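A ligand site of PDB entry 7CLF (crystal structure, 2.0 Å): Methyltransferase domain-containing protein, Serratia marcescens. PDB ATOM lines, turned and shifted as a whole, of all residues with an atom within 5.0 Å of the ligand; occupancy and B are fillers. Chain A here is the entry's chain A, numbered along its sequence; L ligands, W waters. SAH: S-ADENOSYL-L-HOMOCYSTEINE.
Phe 132 touches the ligand (CE2 to C8, 3.5 Å). Leu 149 touches the ligand (CD1 to SD, 3.4 Å). CB of Ala 153 touches OXT of the ligand, at 3.7 Å. Ser 177 touches the ligand. Gly 178 touches the ligand. CD2 of Leu 200 touches C6 of the ligand, 3.5 Å away. Ile 228 touches the ligand. Trp 244 touches the ligand. Met 245 touches the ligand (CG to O4', 3.3 Å).
NE2 of Gln 146 sits at hydrogen-bond distance from OH of Tyr 136, 3.0 Å away. The side-chain carboxylate (OE1) of Glu 199 sits at hydrogen-bond distance from the backbone NH (N) of Gly 178 (2.9 Å). O of Glu 199 lies within hydrogen-bond range of N of Gly 225, at 3.0 Å. The backbone NH (N) of Gly 176 sits at hydrogen-bond distance from the backbone carbonyl oxygen (O) of Cys 198 (2.8 Å). The backbone NH of Ile 228 lies within hydrogen-bond range of the side-chain carboxylate of Asp 226 (2.8 Å).
Water W2 lies within hydrogen-bond range of an oxygen (OXT) of the ligand and the backbone carbonyl oxygen of Leu 149. Water W5 lies within hydrogen-bond range of O of Ile 175 (2.6 Å), N of Gly 243 (2.7 Å), N of the ligand (3.0 Å) and O of Gly 176 (3.4 Å). Water W4 lies within hydrogen-bond range of the backbone carbonyl oxygen of Leu 149 (2.9 Å), an oxygen (OXT) of the ligand (3.1 Å) and the guanidinium group of Arg 331 (3.5 Å).
OH of Tyr 136 sits at hydrogen-bond distance from O2' of the ligand (2.6 Å). The side-chain hydroxyl of Tyr 249 is in hydrogen-bond range of a nitrogen (N7) of the ligand, at 2.6 Å. OE1 of Glu 199 lies within hydrogen-bond range of O3' of the ligand (2.7 Å). The backbone carbonyl oxygen (O) of Gly 243 is in hydrogen-bond range of a nitrogen (N) of the ligand. O of Gly 176 lies within hydrogen-bond range of N of the ligand (2.8 Å). The guanidinium group of Arg 331 is in salt-bridge range of an oxygen (O) of the ligand (2.9 Å). The side-chain carboxylate of Asp 226 is in hydrogen-bond range of a nitrogen (N6) of the ligand. The side-chain amide nitrogen (NE2) of Gln 146 sits at hydrogen-bond distance from an oxygen (O3') of the ligand. N1 of the ligand is in hydrogen-bond range of N of Val 227, 3.1 Å away.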
ATOM      1  N   PHE A 132       3.708 -20.175   0.905  1.00  0.00           N
ATOM      2  CA  PHE A 132       2.915 -20.588   2.056  1.00  0.00           C
ATOM      3  C   PHE A 132       1.583 -19.841   2.126  1.00  0.00           C
ATOM      4  O   PHE A 132       0.587 -20.425   2.539  1.00  0.00           O
ATOM      5  CB  PHE A 132       3.737 -20.455   3.329  1.00  0.00           C
ATOM      6  CG  PHE A 132       4.767 -21.528   3.458  1.00  0.00           C
ATOM      7  CD1 PHE A 132       4.372 -22.837   3.804  1.00  0.00           C
ATOM      8  CD2 PHE A 132       6.103 -21.286   3.193  1.00  0.00           C
ATOM      9  CE1 PHE A 132       5.312 -23.858   3.915  1.00  0.00           C
ATOM     10  CE2 PHE A 132       7.034 -22.297   3.301  1.00  0.00           C
ATOM     11  CZ  PHE A 132       6.630 -23.600   3.666  1.00  0.00           C
ATOM     12  N   TYR A 136      -1.681 -22.006   2.079  1.00  0.00           N
ATOM     13  CA  TYR A 136      -2.486 -21.869   3.281  1.00  0.00           C
ATOM     14  C   TYR A 136      -3.754 -21.043   3.077  1.00  0.00           C
ATOM     15  O   TYR A 136      -4.384 -20.683   4.069  1.00  0.00           O
ATOM     16  CB  TYR A 136      -1.657 -21.241   4.395  1.00  0.00           C
ATOM     17  CG  TYR A 136      -0.547 -22.095   4.970  1.00  0.00           C
ATOM     18  CD1 TYR A 136      -0.420 -23.447   4.647  1.00  0.00           C
ATOM     19  CD2 TYR A 136       0.369 -21.570   5.870  1.00  0.00           C
ATOM     20  CE1 TYR A 136       0.574 -24.229   5.194  1.00  0.00           C
ATOM     21  CE2 TYR A 136       1.371 -22.342   6.423  1.00  0.00           C
ATOM     22  CZ  TYR A 136       1.467 -23.670   6.076  1.00  0.00           C
ATOM     23  OH  TYR A 136       2.469 -24.422   6.633  1.00  0.00           O
ATOM     24  N   PHE A 145      -1.798 -30.529   3.835  1.00  0.00           N
ATOM     25  CA  PHE A 145      -0.352 -30.399   3.877  1.00  0.00           C
ATOM     26  C   PHE A 145       0.209 -30.862   5.217  1.00  0.00           C
ATOM     27  O   PHE A 145       1.126 -31.692   5.271  1.00  0.00           O
ATOM     28  CB  PHE A 145       0.024 -28.931   3.608  1.00  0.00           C
ATOM     29  CG  PHE A 145       1.490 -28.657   3.527  1.00  0.00           C
ATOM     30  CD1 PHE A 145       2.242 -29.120   2.443  1.00  0.00           C
ATOM     31  CD2 PHE A 145       2.126 -27.909   4.509  1.00  0.00           C
ATOM     32  CE1 PHE A 145       3.593 -28.850   2.366  1.00  0.00           C
ATOM     33  CE2 PHE A 145       3.476 -27.639   4.432  1.00  0.00           C
ATOM     34  CZ  PHE A 145       4.201 -28.114   3.354  1.00  0.00           C
ATOM     35  N   GLN A 146      -0.342 -30.347   6.318  1.00  0.00           N
ATOM     36  CA  GLN A 146       0.173 -30.714   7.627  1.00  0.00           C
ATOM     37  C   GLN A 146      -0.097 -32.179   7.955  1.00  0.00           C
ATOM     38  O   GLN A 146       0.705 -32.817   8.642  1.00  0.00           O
ATOM     39  CB  GLN A 146      -0.434 -29.811   8.711  1.00  0.00           C
ATOM     40  CG  GLN A 146      -0.049 -28.327   8.636  1.00  0.00           C
ATOM     41  CD  GLN A 146       1.452 -28.083   8.615  1.00  0.00           C
ATOM     42  OE1 GLN A 146       2.241 -28.921   9.048  1.00  0.00           O
ATOM     43  NE2 GLN A 146       1.868 -26.911   8.127  1.00  0.00           N
ATOM     44  N   LEU A 149       2.471 -34.395   5.826  1.00  0.00           N
ATOM     45  CA  LEU A 149       3.820 -34.218   6.345  1.00  0.00           C
ATOM     46  C   LEU A 149       3.976 -34.889   7.711  1.00  0.00           C
ATOM     47  O   LEU A 149       5.022 -35.472   7.999  1.00  0.00           O
ATOM     48  CB  LEU A 149       4.165 -32.729   6.470  1.00  0.00           C
ATOM     49  CG  LEU A 149       4.540 -31.952   5.212  1.00  0.00           C
ATOM     50  CD1 LEU A 149       4.882 -30.557   5.642  1.00  0.00           C
ATOM     51  CD2 LEU A 149       5.710 -32.576   4.471  1.00  0.00           C
ATOM     52  N   ALA A 153       6.825 -37.598   8.918  1.00  0.00           N
ATOM     53  CA  ALA A 153       7.768 -37.241   9.976  1.00  0.00           C
ATOM     54  C   ALA A 153       7.759 -38.226  11.143  1.00  0.00           C
ATOM     55  O   ALA A 153       8.631 -38.142  12.005  1.00  0.00           O
ATOM     56  CB  ALA A 153       7.471 -35.830  10.516  1.00  0.00           C
ATOM     57  N   PHE A 156      11.167 -40.147  11.929  1.00  0.00           N
ATOM     58  CA  PHE A 156      12.126 -39.192  12.470  1.00  0.00           C
ATOM     59  C   PHE A 156      11.822 -38.855  13.930  1.00  0.00           C
ATOM     60  O   PHE A 156      12.691 -38.934  14.795  1.00  0.00           O
ATOM     61  CB  PHE A 156      12.125 -37.909  11.631  1.00  0.00           C
ATOM     62  CG  PHE A 156      12.692 -36.712  12.358  1.00  0.00           C
ATOM     63  CD1 PHE A 156      14.033 -36.655  12.688  1.00  0.00           C
ATOM     64  CD2 PHE A 156      11.889 -35.642  12.692  1.00  0.00           C
ATOM     65  CE1 PHE A 156      14.560 -35.559  13.350  1.00  0.00           C
ATOM     66  CE2 PHE A 156      12.397 -34.539  13.368  1.00  0.00           C
ATOM     67  CZ  PHE A 156      13.730 -34.502  13.690  1.00  0.00           C
ATOM     68  N   ILE A 175      10.314 -24.289  15.956  1.00  0.00           N
ATOM     69  CA  ILE A 175       9.998 -23.269  14.950  1.00  0.00           C
ATOM     70  C   ILE A 175       9.567 -23.982  13.682  1.00  0.00           C
ATOM     71  O   ILE A 175      10.315 -24.804  13.144  1.00  0.00           O
ATOM     72  CB  ILE A 175      11.202 -22.349  14.681  1.00  0.00           C
ATOM     73  CG1 ILE A 175      11.540 -21.485  15.890  1.00  0.00           C
ATOM     74  CG2 ILE A 175      10.916 -21.483  13.454  1.00  0.00           C
ATOM     75  CD1 ILE A 175      12.759 -20.575  15.674  1.00  0.00           C
ATOM     76  N   GLY A 176       8.373 -23.672  13.190  1.00  0.00           N
ATOM     77  CA  GLY A 176       7.866 -24.341  12.004  1.00  0.00           C
ATOM     78  C   GLY A 176       7.424 -25.767  12.255  1.00  0.00           C
ATOM     79  O   GLY A 176       7.503 -26.603  11.352  1.00  0.00           O
ATOM     80  N   SER A 177       6.948 -26.051  13.468  1.00  0.00           N
ATOM     81  CA  SER A 177       6.609 -27.403  13.895  1.00  0.00           C
ATOM     82  C   SER A 177       5.580 -28.060  12.976  1.00  0.00           C
ATOM     83  O   SER A 177       5.547 -29.283  12.879  1.00  0.00           O
ATOM     84  CB  SER A 177       6.101 -27.352  15.338  1.00  0.00           C
ATOM     85  OG  SER A 177       5.933 -28.645  15.918  1.00  0.00           O
ATOM     86  N   GLY A 178       4.739 -27.276  12.318  1.00  0.00           N
ATOM     87  CA  GLY A 178       3.761 -27.835  11.424  1.00  0.00           C
ATOM     88  C   GLY A 178       2.554 -28.386  12.144  1.00  0.00           C
ATOM     89  O   GLY A 178       1.748 -27.629  12.695  1.00  0.00           O
ATOM     90  N   CYS A 198       6.489 -22.009  17.302  1.00  0.00           N
ATOM     91  CA  CYS A 198       6.405 -20.763  16.550  1.00  0.00           C
ATOM     92  C   CYS A 198       6.027 -21.070  15.109  1.00  0.00           C
ATOM     93  O   CYS A 198       6.789 -21.739  14.399  1.00  0.00           O
ATOM     94  CB  CYS A 198       7.711 -19.984  16.577  1.00  0.00           C
ATOM     95  SG  CYS A 198       7.451 -18.372  15.796  1.00  0.00           S
ATOM     96  N   GLU A 199       4.864 -20.595  14.666  1.00  0.00           N
ATOM     97  CA  GLU A 199       4.389 -20.934  13.338  1.00  0.00           C
ATOM     98  C   GLU A 199       3.779 -19.721  12.646  1.00  0.00           C
ATOM     99  O   GLU A 199       3.475 -18.701  13.272  1.00  0.00           O
ATOM    100  CB  GLU A 199       3.378 -22.081  13.371  1.00  0.00           C
ATOM    101  CG  GLU A 199       3.986 -23.420  12.983  1.00  0.00           C
ATOM    102  CD  GLU A 199       4.190 -23.579  11.477  1.00  0.00           C
ATOM    103  OE1 GLU A 199       4.549 -24.698  11.072  1.00  0.00           O
ATOM    104  OE2 GLU A 199       3.995 -22.606  10.704  1.00  0.00           O
ATOM    105  N   LEU A 200       3.630 -19.851  11.331  1.00  0.00           N
ATOM    106  CA  LEU A 200       2.933 -18.847  10.540  1.00  0.00           C
ATOM    107  C   LEU A 200       1.457 -18.800  10.932  1.00  0.00           C
ATOM    108  O   LEU A 200       0.922 -19.764  11.496  1.00  0.00           O
ATOM    109  CB  LEU A 200       3.095 -19.143   9.054  1.00  0.00           C
ATOM    110  CG  LEU A 200       4.491 -19.037   8.472  1.00  0.00           C
ATOM    111  CD1 LEU A 200       4.497 -19.495   7.020  1.00  0.00           C
ATOM    112  CD2 LEU A 200       5.044 -17.612   8.584  1.00  0.00           C
ATOM    113  N   ALA A 203      -1.091 -21.635   9.882  1.00  0.00           N
ATOM    114  CA  ALA A 203      -0.752 -22.924  10.455  1.00  0.00           C
ATOM    115  C   ALA A 203      -0.923 -22.907  11.965  1.00  0.00           C
ATOM    116  O   ALA A 203      -1.301 -23.922  12.549  1.00  0.00           O
ATOM    117  CB  ALA A 203       0.672 -23.330  10.071  1.00  0.00           C
ATOM    118  N   GLY A 225       4.560 -16.218  14.448  1.00  0.00           N
ATOM    119  CA  GLY A 225       5.763 -15.468  14.158  1.00  0.00           C
ATOM    120  C   GLY A 225       6.193 -15.643  12.718  1.00  0.00           C
ATOM    121  O   GLY A 225       5.468 -16.196  11.884  1.00  0.00           O
ATOM    122  N   ASP A 226       7.400 -15.140  12.452  1.00  0.00           N
ATOM    123  CA  ASP A 226       8.016 -15.262  11.137  1.00  0.00           C
ATOM    124  C   ASP A 226       9.516 -15.296  11.376  1.00  0.00           C
ATOM    125  O   ASP A 226      10.087 -14.310  11.857  1.00  0.00           O
ATOM    126  CB  ASP A 226       7.613 -14.097  10.226  1.00  0.00           C
ATOM    127  CG  ASP A 226       8.184 -14.215   8.828  1.00  0.00           C
ATOM    128  OD1 ASP A 226       9.091 -15.054   8.585  1.00  0.00           O
ATOM    129  OD2 ASP A 226       7.714 -13.448   7.968  1.00  0.00           O
ATOM    130  N   VAL A 227      10.149 -16.423  11.053  1.00  0.00           N
ATOM    131  CA  VAL A 227      11.577 -16.576  11.322  1.00  0.00           C
ATOM    132  C   VAL A 227      12.416 -15.803  10.322  1.00  0.00           C
ATOM    133  O   VAL A 227      13.596 -15.534  10.579  1.00  0.00           O
ATOM    134  CB  VAL A 227      11.938 -18.084  11.344  1.00  0.00           C
ATOM    135  CG1 VAL A 227      11.747 -18.701   9.961  1.00  0.00           C
ATOM    136  CG2 VAL A 227      13.363 -18.298  11.844  1.00  0.00           C
ATOM    137  N   ILE A 228      11.843 -15.415   9.182  1.00  0.00           N
ATOM    138  CA  ILE A 228      12.591 -14.637   8.202  1.00  0.00           C
ATOM    139  C   ILE A 228      12.586 -13.158   8.570  1.00  0.00           C
ATOM    140  O   ILE A 228      13.581 -12.467   8.362  1.00  0.00           O
ATOM    141  CB  ILE A 228      12.032 -14.872   6.790  1.00  0.00           C
ATOM    142  CG1 ILE A 228      12.082 -16.350   6.424  1.00  0.00           C
ATOM    143  CG2 ILE A 228      12.826 -14.066   5.772  1.00  0.00           C
ATOM    144  CD1 ILE A 228      11.269 -16.648   5.218  1.00  0.00           C
ATOM    145  N   GLY A 243      12.604 -27.977  11.863  1.00  0.00           N
ATOM    146  CA  GLY A 243      12.537 -29.215  11.094  1.00  0.00           C
ATOM    147  C   GLY A 243      11.984 -29.077   9.698  1.00  0.00           C
ATOM    148  O   GLY A 243      10.844 -28.674   9.497  1.00  0.00           O
ATOM    149  N   TRP A 244      12.788 -29.435   8.721  1.00  0.00           N
ATOM    150  CA  TRP A 244      12.297 -29.466   7.315  1.00  0.00           C
ATOM    151  C   TRP A 244      11.792 -28.114   6.824  1.00  0.00           C
ATOM    152  O   TRP A 244      10.836 -28.098   6.131  1.00  0.00           O
ATOM    153  CB  TRP A 244      11.294 -30.599   7.146  1.00  0.00           C
ATOM    154  CG  TRP A 244      11.809 -31.615   6.175  1.00  0.00           C
ATOM    155  CD1 TRP A 244      13.116 -31.829   5.842  1.00  0.00           C
ATOM    156  CD2 TRP A 244      11.043 -32.509   5.370  1.00  0.00           C
ATOM    157  NE1 TRP A 244      13.209 -32.796   4.877  1.00  0.00           N
ATOM    158  CE2 TRP A 244      11.944 -33.230   4.566  1.00  0.00           C
ATOM    159  CE3 TRP A 244       9.684 -32.750   5.217  1.00  0.00           C
ATOM    160  CZ2 TRP A 244      11.529 -34.188   3.655  1.00  0.00           C
ATOM    161  CZ3 TRP A 244       9.263 -33.700   4.316  1.00  0.00           C
ATOM    162  CH2 TRP A 244      10.181 -34.406   3.546  1.00  0.00           C
ATOM    163  N   MET A 245      12.437 -27.021   7.226  1.00  0.00           N
ATOM    164  CA  MET A 245      12.044 -25.696   6.735  1.00  0.00           C
ATOM    165  C   MET A 245      13.127 -25.000   5.926  1.00  0.00           C
ATOM    166  O   MET A 245      12.793 -24.232   5.025  1.00  0.00           O
ATOM    167  CB  MET A 245      11.635 -24.781   7.897  1.00  0.00           C
ATOM    168  CG  MET A 245      10.681 -23.704   7.462  1.00  0.00           C
ATOM    169  SD  MET A 245      11.017 -22.170   8.321  1.00  0.00           S
ATOM    170  CE  MET A 245      12.721 -22.049   7.868  1.00  0.00           C
ATOM    171  N   ASP A 248      12.932 -25.005   2.137  1.00  0.00           N
ATOM    172  CA  ASP A 248      11.864 -24.285   1.468  1.00  0.00           C
ATOM    173  C   ASP A 248      12.291 -22.882   1.053  1.00  0.00           C
ATOM    174  O   ASP A 248      11.452 -22.116   0.555  1.00  0.00           O
ATOM    175  CB  ASP A 248      10.629 -24.221   2.381  1.00  0.00           C
ATOM    176  CG  ASP A 248       9.944 -25.572   2.522  1.00  0.00           C
ATOM    177  OD1 ASP A 248       9.734 -26.242   1.502  1.00  0.00           O
ATOM    178  OD2 ASP A 248       9.635 -25.972   3.667  1.00  0.00           O
ATOM    179  N   TYR A 249      13.567 -22.536   1.227  1.00  0.00           N
ATOM    180  CA  TYR A 249      14.038 -21.177   0.956  1.00  0.00           C
ATOM    181  C   TYR A 249      15.420 -21.189   0.344  1.00  0.00           C
ATOM    182  O   TYR A 249      16.208 -22.113   0.517  1.00  0.00           O
ATOM    183  CB  TYR A 249      14.059 -20.325   2.242  1.00  0.00           C
ATOM    184  CG  TYR A 249      12.696 -20.094   2.825  1.00  0.00           C
ATOM    185  CD1 TYR A 249      11.823 -19.202   2.239  1.00  0.00           C
ATOM    186  CD2 TYR A 249      12.280 -20.780   3.961  1.00  0.00           C
ATOM    187  CE1 TYR A 249      10.566 -18.981   2.774  1.00  0.00           C
ATOM    188  CE2 TYR A 249      11.018 -20.570   4.503  1.00  0.00           C
ATOM    189  CZ  TYR A 249      10.172 -19.656   3.913  1.00  0.00           C
ATOM    190  OH  TYR A 249       8.924 -19.422   4.433  1.00  0.00           O
ATOM    191  N   ARG A 331      16.747 -38.357   8.974  1.00  0.00           N
ATOM    192  CA  ARG A 331      17.228 -37.003   8.789  1.00  0.00           C
ATOM    193  C   ARG A 331      18.665 -36.858   9.270  1.00  0.00           C
ATOM    194  O   ARG A 331      19.181 -37.696  10.015  1.00  0.00           O
ATOM    195  CB  ARG A 331      16.334 -35.998   9.535  1.00  0.00           C
ATOM    196  CG  ARG A 331      14.876 -36.013   9.067  1.00  0.00           C
ATOM    197  CD  ARG A 331      14.122 -34.778   9.563  1.00  0.00           C
ATOM    198  NE  ARG A 331      12.700 -34.814   9.215  1.00  0.00           N
ATOM    199  CZ  ARG A 331      11.830 -33.903   9.632  1.00  0.00           C
ATOM    200  NH1 ARG A 331      12.237 -32.899  10.396  1.00  0.00           N
ATOM    201  NH2 ARG A 331      10.552 -33.995   9.285  1.00  0.00           N
HETATM  202  N   SAH L   1       8.682 -29.177  11.202  1.00  0.00           N
HETATM  203  CA  SAH L   1       7.740 -30.082  10.552  1.00  0.00           C
HETATM  204  CB  SAH L   1       7.073 -29.428   9.328  1.00  0.00           C
HETATM  205  CG  SAH L   1       7.945 -28.931   8.167  1.00  0.00           C
HETATM  206  SD  SAH L   1       6.955 -28.099   6.866  1.00  0.00           S
HETATM  207  C   SAH L   1       8.459 -31.370  10.177  1.00  0.00           C
HETATM  208  O   SAH L   1       9.634 -31.551  10.509  1.00  0.00           O
HETATM  209  OXT SAH L   1       7.879 -32.248   9.538  1.00  0.00           O
HETATM  210  C5' SAH L   1       7.702 -26.468   7.172  1.00  0.00           C
HETATM  211  C4' SAH L   1       6.928 -25.607   8.179  1.00  0.00           C
HETATM  212  O4' SAH L   1       7.612 -24.369   8.340  1.00  0.00           O
HETATM  213  C3' SAH L   1       5.529 -25.292   7.689  1.00  0.00           C
HETATM  214  O3' SAH L   1       4.588 -25.723   8.627  1.00  0.00           O
HETATM  215  C2' SAH L   1       5.503 -23.781   7.576  1.00  0.00           C
HETATM  216  O2' SAH L   1       4.288 -23.217   8.014  1.00  0.00           O
HETATM  217  C1' SAH L   1       6.663 -23.333   8.435  1.00  0.00           C
HETATM  218  N9  SAH L   1       7.230 -22.068   7.956  1.00  0.00           N
HETATM  219  C8  SAH L   1       7.555 -21.714   6.672  1.00  0.00           C
HETATM  220  N7  SAH L   1       8.043 -20.453   6.671  1.00  0.00           N
HETATM  221  C5  SAH L   1       8.013 -19.984   7.938  1.00  0.00           C
HETATM  222  C6  SAH L   1       8.394 -18.770   8.484  1.00  0.00           C
HETATM  223  N6  SAH L   1       8.885 -17.810   7.708  1.00  0.00           N
HETATM  224  N1  SAH L   1       8.249 -18.574   9.844  1.00  0.00           N
HETATM  225  C2  SAH L   1       7.746 -19.578  10.639  1.00  0.00           C
HETATM  226  N3  SAH L   1       7.369 -20.790  10.085  1.00  0.00           N
HETATM  227  C4  SAH L   1       7.508 -20.982   8.757  1.00  0.00           C
HETATM  228  O   HOH W   1       9.219 -30.387  13.850  1.00  0.00           O
HETATM  229  O   HOH W   2       5.293 -32.878  10.286  1.00  0.00           O
HETATM  230  O   HOH W   3       9.056 -32.941  13.046  1.00  0.00           O
HETATM  231  O   HOH W   4       7.708 -34.516   7.380  1.00  0.00           O
HETATM  232  O   HOH W   5      10.300 -27.428  13.106  1.00  0.00           O
